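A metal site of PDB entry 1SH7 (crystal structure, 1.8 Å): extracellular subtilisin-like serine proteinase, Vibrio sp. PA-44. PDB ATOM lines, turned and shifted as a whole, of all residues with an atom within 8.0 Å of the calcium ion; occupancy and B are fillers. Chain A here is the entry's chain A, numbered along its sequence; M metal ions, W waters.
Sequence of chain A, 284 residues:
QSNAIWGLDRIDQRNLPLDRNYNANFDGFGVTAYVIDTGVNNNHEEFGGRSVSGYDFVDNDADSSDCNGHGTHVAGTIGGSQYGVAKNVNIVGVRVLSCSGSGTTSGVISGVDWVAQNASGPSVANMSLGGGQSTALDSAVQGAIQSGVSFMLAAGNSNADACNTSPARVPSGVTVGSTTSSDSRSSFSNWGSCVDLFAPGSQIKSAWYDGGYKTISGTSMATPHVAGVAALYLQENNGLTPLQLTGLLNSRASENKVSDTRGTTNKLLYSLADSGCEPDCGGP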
ATOM      1  N   PHE A 151      17.155  -5.822  -9.978  1.00  0.00           N
ATOM      2  CA  PHE A 151      16.992  -7.201 -10.357  1.00  0.00           C
ATOM      3  C   PHE A 151      17.975  -7.564 -11.462  1.00  0.00           C
ATOM      4  O   PHE A 151      17.950  -6.927 -12.544  1.00  0.00           O
ATOM      5  CB  PHE A 151      15.559  -7.487 -10.826  1.00  0.00           C
ATOM      6  CG  PHE A 151      14.611  -7.909  -9.710  1.00  0.00           C
ATOM      7  CD1 PHE A 151      14.270  -7.013  -8.704  1.00  0.00           C
ATOM      8  CD2 PHE A 151      14.099  -9.179  -9.670  1.00  0.00           C
ATOM      9  CE1 PHE A 151      13.463  -7.365  -7.666  1.00  0.00           C
ATOM     10  CE2 PHE A 151      13.269  -9.566  -8.661  1.00  0.00           C
ATOM     11  CZ  PHE A 151      12.928  -8.652  -7.642  1.00  0.00           C
ATOM     12  N   LEU A 153      18.991 -10.532 -14.089  1.00  0.00           N
ATOM     13  CA  LEU A 153      18.196 -11.538 -14.813  1.00  0.00           C
ATOM     14  C   LEU A 153      19.058 -12.292 -15.820  1.00  0.00           C
ATOM     15  O   LEU A 153      19.792 -11.664 -16.564  1.00  0.00           O
ATOM     16  CB  LEU A 153      17.054 -10.828 -15.574  1.00  0.00           C
ATOM     17  CG  LEU A 153      16.252  -9.824 -14.752  1.00  0.00           C
ATOM     18  CD1 LEU A 153      15.297  -9.032 -15.657  1.00  0.00           C
ATOM     19  CD2 LEU A 153      15.505 -10.495 -13.631  1.00  0.00           C
ATOM     20  N   ALA A 168      13.912 -12.072 -18.626  1.00  0.00           N
ATOM     21  CA  ALA A 168      15.043 -11.382 -19.302  1.00  0.00           C
ATOM     22  C   ALA A 168      14.689 -10.111 -20.059  1.00  0.00           C
ATOM     23  O   ALA A 168      15.477  -9.139 -20.097  1.00  0.00           O
ATOM     24  CB  ALA A 168      15.733 -12.330 -20.265  1.00  0.00           C
ATOM     25  N   ARG A 169      13.543 -10.119 -20.708  1.00  0.00           N
ATOM     26  CA  ARG A 169      13.189  -9.028 -21.582  1.00  0.00           C
ATOM     27  C   ARG A 169      12.716  -7.772 -20.856  1.00  0.00           C
ATOM     28  O   ARG A 169      12.618  -6.726 -21.487  1.00  0.00           O
ATOM     29  CB  ARG A 169      12.160  -9.494 -22.604  1.00  0.00           C
ATOM     30  CG  ARG A 169      10.785  -9.782 -22.031  1.00  0.00           C
ATOM     31  CD  ARG A 169       9.850 -10.263 -23.101  1.00  0.00           C
ATOM     32  NE  ARG A 169       8.487 -10.331 -22.646  1.00  0.00           N
ATOM     33  CZ  ARG A 169       7.466  -9.796 -23.271  1.00  0.00           C
ATOM     34  NH1 ARG A 169       7.627  -9.109 -24.408  1.00  0.00           N
ATOM     35  NH2 ARG A 169       6.251  -9.968 -22.764  1.00  0.00           N
ATOM     36  N   VAL A 170      12.449  -7.842 -19.551  1.00  0.00           N
ATOM     37  CA  VAL A 170      11.976  -6.653 -18.795  1.00  0.00           C
ATOM     38  C   VAL A 170      12.980  -5.520 -18.910  1.00  0.00           C
ATOM     39  O   VAL A 170      14.106  -5.634 -18.395  1.00  0.00           O
ATOM     40  CB  VAL A 170      11.760  -6.984 -17.306  1.00  0.00           C
ATOM     41  CG1 VAL A 170      11.510  -5.713 -16.472  1.00  0.00           C
ATOM     42  CG2 VAL A 170      10.582  -7.928 -17.121  1.00  0.00           C
ATOM     43  N   PRO A 171      12.625  -4.436 -19.617  1.00  0.00           N
ATOM     44  CA  PRO A 171      13.625  -3.396 -19.851  1.00  0.00           C
ATOM     45  C   PRO A 171      14.382  -2.959 -18.604  1.00  0.00           C
ATOM     46  O   PRO A 171      15.597  -2.906 -18.664  1.00  0.00           O
ATOM     47  CB  PRO A 171      12.797  -2.269 -20.477  1.00  0.00           C
ATOM     48  CG  PRO A 171      11.694  -3.020 -21.212  1.00  0.00           C
ATOM     49  CD  PRO A 171      11.353  -4.118 -20.303  1.00  0.00           C
ATOM     50  N   SER A 172      13.724  -2.723 -17.472  1.00  0.00           N
ATOM     51  CA  SER A 172      14.398  -2.109 -16.297  1.00  0.00           C
ATOM     52  C   SER A 172      15.232  -3.085 -15.441  1.00  0.00           C
ATOM     53  O   SER A 172      15.879  -2.711 -14.473  1.00  0.00           O
ATOM     54  CB  SER A 172      13.412  -1.311 -15.460  1.00  0.00           C
ATOM     55  OG  SER A 172      12.451  -2.158 -14.881  1.00  0.00           O
ATOM     56  N   GLY A 173      15.231  -4.339 -15.843  1.00  0.00           N
ATOM     57  CA  GLY A 173      16.090  -5.347 -15.283  1.00  0.00           C
ATOM     58  C   GLY A 173      17.448  -5.238 -15.917  1.00  0.00           C
ATOM     59  O   GLY A 173      17.603  -4.654 -16.985  1.00  0.00           O
ATOM     60  N   VAL A 174      18.447  -5.806 -15.234  1.00  0.00           N
ATOM     61  CA  VAL A 174      19.781  -5.917 -15.760  1.00  0.00           C
ATOM     62  C   VAL A 174      19.945  -7.346 -16.221  1.00  0.00           C
ATOM     63  O   VAL A 174      20.030  -8.265 -15.384  1.00  0.00           O
ATOM     64  CB  VAL A 174      20.845  -5.575 -14.717  1.00  0.00           C
ATOM     65  CG1 VAL A 174      22.213  -5.665 -15.348  1.00  0.00           C
ATOM     66  CG2 VAL A 174      20.612  -4.175 -14.097  1.00  0.00           C
ATOM     67  N   THR A 175      19.959  -7.519 -17.541  1.00  0.00           N
ATOM     68  CA  THR A 175      19.885  -8.819 -18.210  1.00  0.00           C
ATOM     69  C   THR A 175      21.289  -9.202 -18.685  1.00  0.00           C
ATOM     70  O   THR A 175      21.967  -8.427 -19.368  1.00  0.00           O
ATOM     71  CB  THR A 175      18.934  -8.709 -19.395  1.00  0.00           C
ATOM     72  OG1 THR A 175      17.631  -8.317 -18.940  1.00  0.00           O
ATOM     73  CG2 THR A 175      18.742 -10.078 -20.112  1.00  0.00           C
ATOM     74  N   VAL A 176      21.720 -10.397 -18.313  1.00  0.00           N
ATOM     75  CA  VAL A 176      23.128 -10.761 -18.363  1.00  0.00           C
ATOM     76  C   VAL A 176      23.384 -11.925 -19.288  1.00  0.00           C
ATOM     77  O   VAL A 176      22.843 -13.013 -19.086  1.00  0.00           O
ATOM     78  CB  VAL A 176      23.617 -11.177 -16.946  1.00  0.00           C
ATOM     79  CG1 VAL A 176      25.151 -11.456 -17.000  1.00  0.00           C
ATOM     80  CG2 VAL A 176      23.254 -10.126 -15.918  1.00  0.00           C
ATOM     81  N   SER A 193      19.318  -6.959 -28.264  1.00  0.00           N
ATOM     82  CA  SER A 193      18.994  -5.653 -27.693  1.00  0.00           C
ATOM     83  C   SER A 193      18.524  -5.679 -26.232  1.00  0.00           C
ATOM     84  O   SER A 193      18.590  -4.642 -25.584  1.00  0.00           O
ATOM     85  CB  SER A 193      17.916  -4.981 -28.532  1.00  0.00           C
ATOM     86  OG  SER A 193      16.711  -5.717 -28.462  1.00  0.00           O
ATOM     87  N   CYS A 194      17.996  -6.802 -25.727  1.00  0.00           N
ATOM     88  CA  CYS A 194      17.518  -6.864 -24.335  1.00  0.00           C
ATOM     89  C   CYS A 194      18.606  -7.222 -23.322  1.00  0.00           C
ATOM     90  O   CYS A 194      18.366  -7.177 -22.133  1.00  0.00           O
ATOM     91  CB  CYS A 194      16.402  -7.866 -24.205  1.00  0.00           C
ATOM     92  SG  CYS A 194      14.882  -7.291 -24.928  1.00  0.00           S
ATOM     93  N   VAL A 195      19.779  -7.625 -23.797  1.00  0.00           N
ATOM     94  CA  VAL A 195      20.917  -8.000 -22.954  1.00  0.00           C
ATOM     95  C   VAL A 195      21.698  -6.721 -22.610  1.00  0.00           C
ATOM     96  O   VAL A 195      22.128  -6.023 -23.507  1.00  0.00           O
ATOM     97  CB  VAL A 195      21.874  -8.966 -23.696  1.00  0.00           C
ATOM     98  CG1 VAL A 195      23.130  -9.240 -22.881  1.00  0.00           C
ATOM     99  CG2 VAL A 195      21.153 -10.261 -24.078  1.00  0.00           C
ATOM    100  N   ASP A 196      21.872  -6.427 -21.323  1.00  0.00           N
ATOM    101  CA  ASP A 196      22.510  -5.200 -20.889  1.00  0.00           C
ATOM    102  C   ASP A 196      24.029  -5.287 -20.852  1.00  0.00           C
ATOM    103  O   ASP A 196      24.692  -4.304 -21.093  1.00  0.00           O
ATOM    104  CB  ASP A 196      22.040  -4.812 -19.491  1.00  0.00           C
ATOM    105  CG  ASP A 196      20.559  -4.441 -19.454  1.00  0.00           C
ATOM    106  OD1 ASP A 196      20.206  -3.304 -19.799  1.00  0.00           O
ATOM    107  OD2 ASP A 196      19.697  -5.224 -19.068  1.00  0.00           O
ATOM    108  N   LEU A 197      24.547  -6.467 -20.518  1.00  0.00           N
ATOM    109  CA  LEU A 197      25.998  -6.702 -20.461  1.00  0.00           C
ATOM    110  C   LEU A 197      26.301  -8.195 -20.342  1.00  0.00           C
ATOM    111  O   LEU A 197      25.392  -8.997 -20.078  1.00  0.00           O
ATOM    112  CB  LEU A 197      26.661  -5.931 -19.291  1.00  0.00           C
ATOM    113  CG  LEU A 197      26.597  -6.513 -17.869  1.00  0.00           C
ATOM    114  CD1 LEU A 197      27.408  -5.727 -16.863  1.00  0.00           C
ATOM    115  CD2 LEU A 197      25.140  -6.555 -17.432  1.00  0.00           C
ATOM    116  N   THR A 246      21.961   0.465 -12.297  1.00  0.00           N
ATOM    117  CA  THR A 246      22.046   0.146 -13.718  1.00  0.00           C
ATOM    118  C   THR A 246      23.030   1.081 -14.441  1.00  0.00           C
ATOM    119  O   THR A 246      23.903   0.621 -15.177  1.00  0.00           O
ATOM    120  CB  THR A 246      20.661   0.230 -14.353  1.00  0.00           C
ATOM    121  OG1 THR A 246      19.861  -0.846 -13.843  1.00  0.00           O
ATOM    122  CG2 THR A 246      20.734   0.053 -15.886  1.00  0.00           C
ATOM    123  N   ASN A 250      26.693  -0.035 -16.222  1.00  0.00           N
ATOM    124  CA  ASN A 250      26.993   0.407 -17.566  1.00  0.00           C
ATOM    125  C   ASN A 250      28.231   1.282 -17.726  1.00  0.00           C
ATOM    126  O   ASN A 250      29.065   1.031 -18.573  1.00  0.00           O
ATOM    127  CB  ASN A 250      25.808   1.195 -18.120  1.00  0.00           C
ATOM    128  CG  ASN A 250      24.783   0.311 -18.753  1.00  0.00           C
ATOM    129  OD1 ASN A 250      24.975  -0.165 -19.877  1.00  0.00           O
ATOM    130  ND2 ASN A 250      23.673   0.082 -18.055  1.00  0.00           N
HETATM  131 CA    CA M   1      17.870  -3.725 -19.164  1.00  0.00          CA
HETATM  132  O   HOH W   1      18.508  -1.883 -17.885  1.00  0.00           O
HETATM  133  O   HOH W   2      17.373  -1.767 -20.698  1.00  0.00           O
HETATM  134  O   HOH W   3      16.581  -5.804 -19.435  1.00  0.00           O
HETATM  135  O   HOH W   4      18.133  -4.466 -21.415  1.00  0.00           O
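O of Thr 175 is in hydrogen-bond range of N of Asp 196.
Of the 18 residues printed, 3 come within 4 Å of the calcium ion.
The nearest printed residue that does not touch the calcium ion is Val 170 (4.3 Å).
Water W1 binds the calcium ion, 2.3 Å away.
The calcium ion is bound by OD2 of Asp 196.
O of Gly 173 is bound to the calcium ion (2.4 Å).
The calcium ion is bound by water W4, at 2.4 Å.
OD1 of Asp 196 is bound to the calcium ion (2.5 Å).
Water W3 is bound to the calcium ion, at 2.5 Å.
The calcium ion is bound by O of Pro 171 (2.5 Å).
Water W2 is bound to the calcium ion (2.5 Å).
The calcium ion has eight donor atoms within binding distance.
Water W3 bridges O of Val 170 and OG1 of Thr 175.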
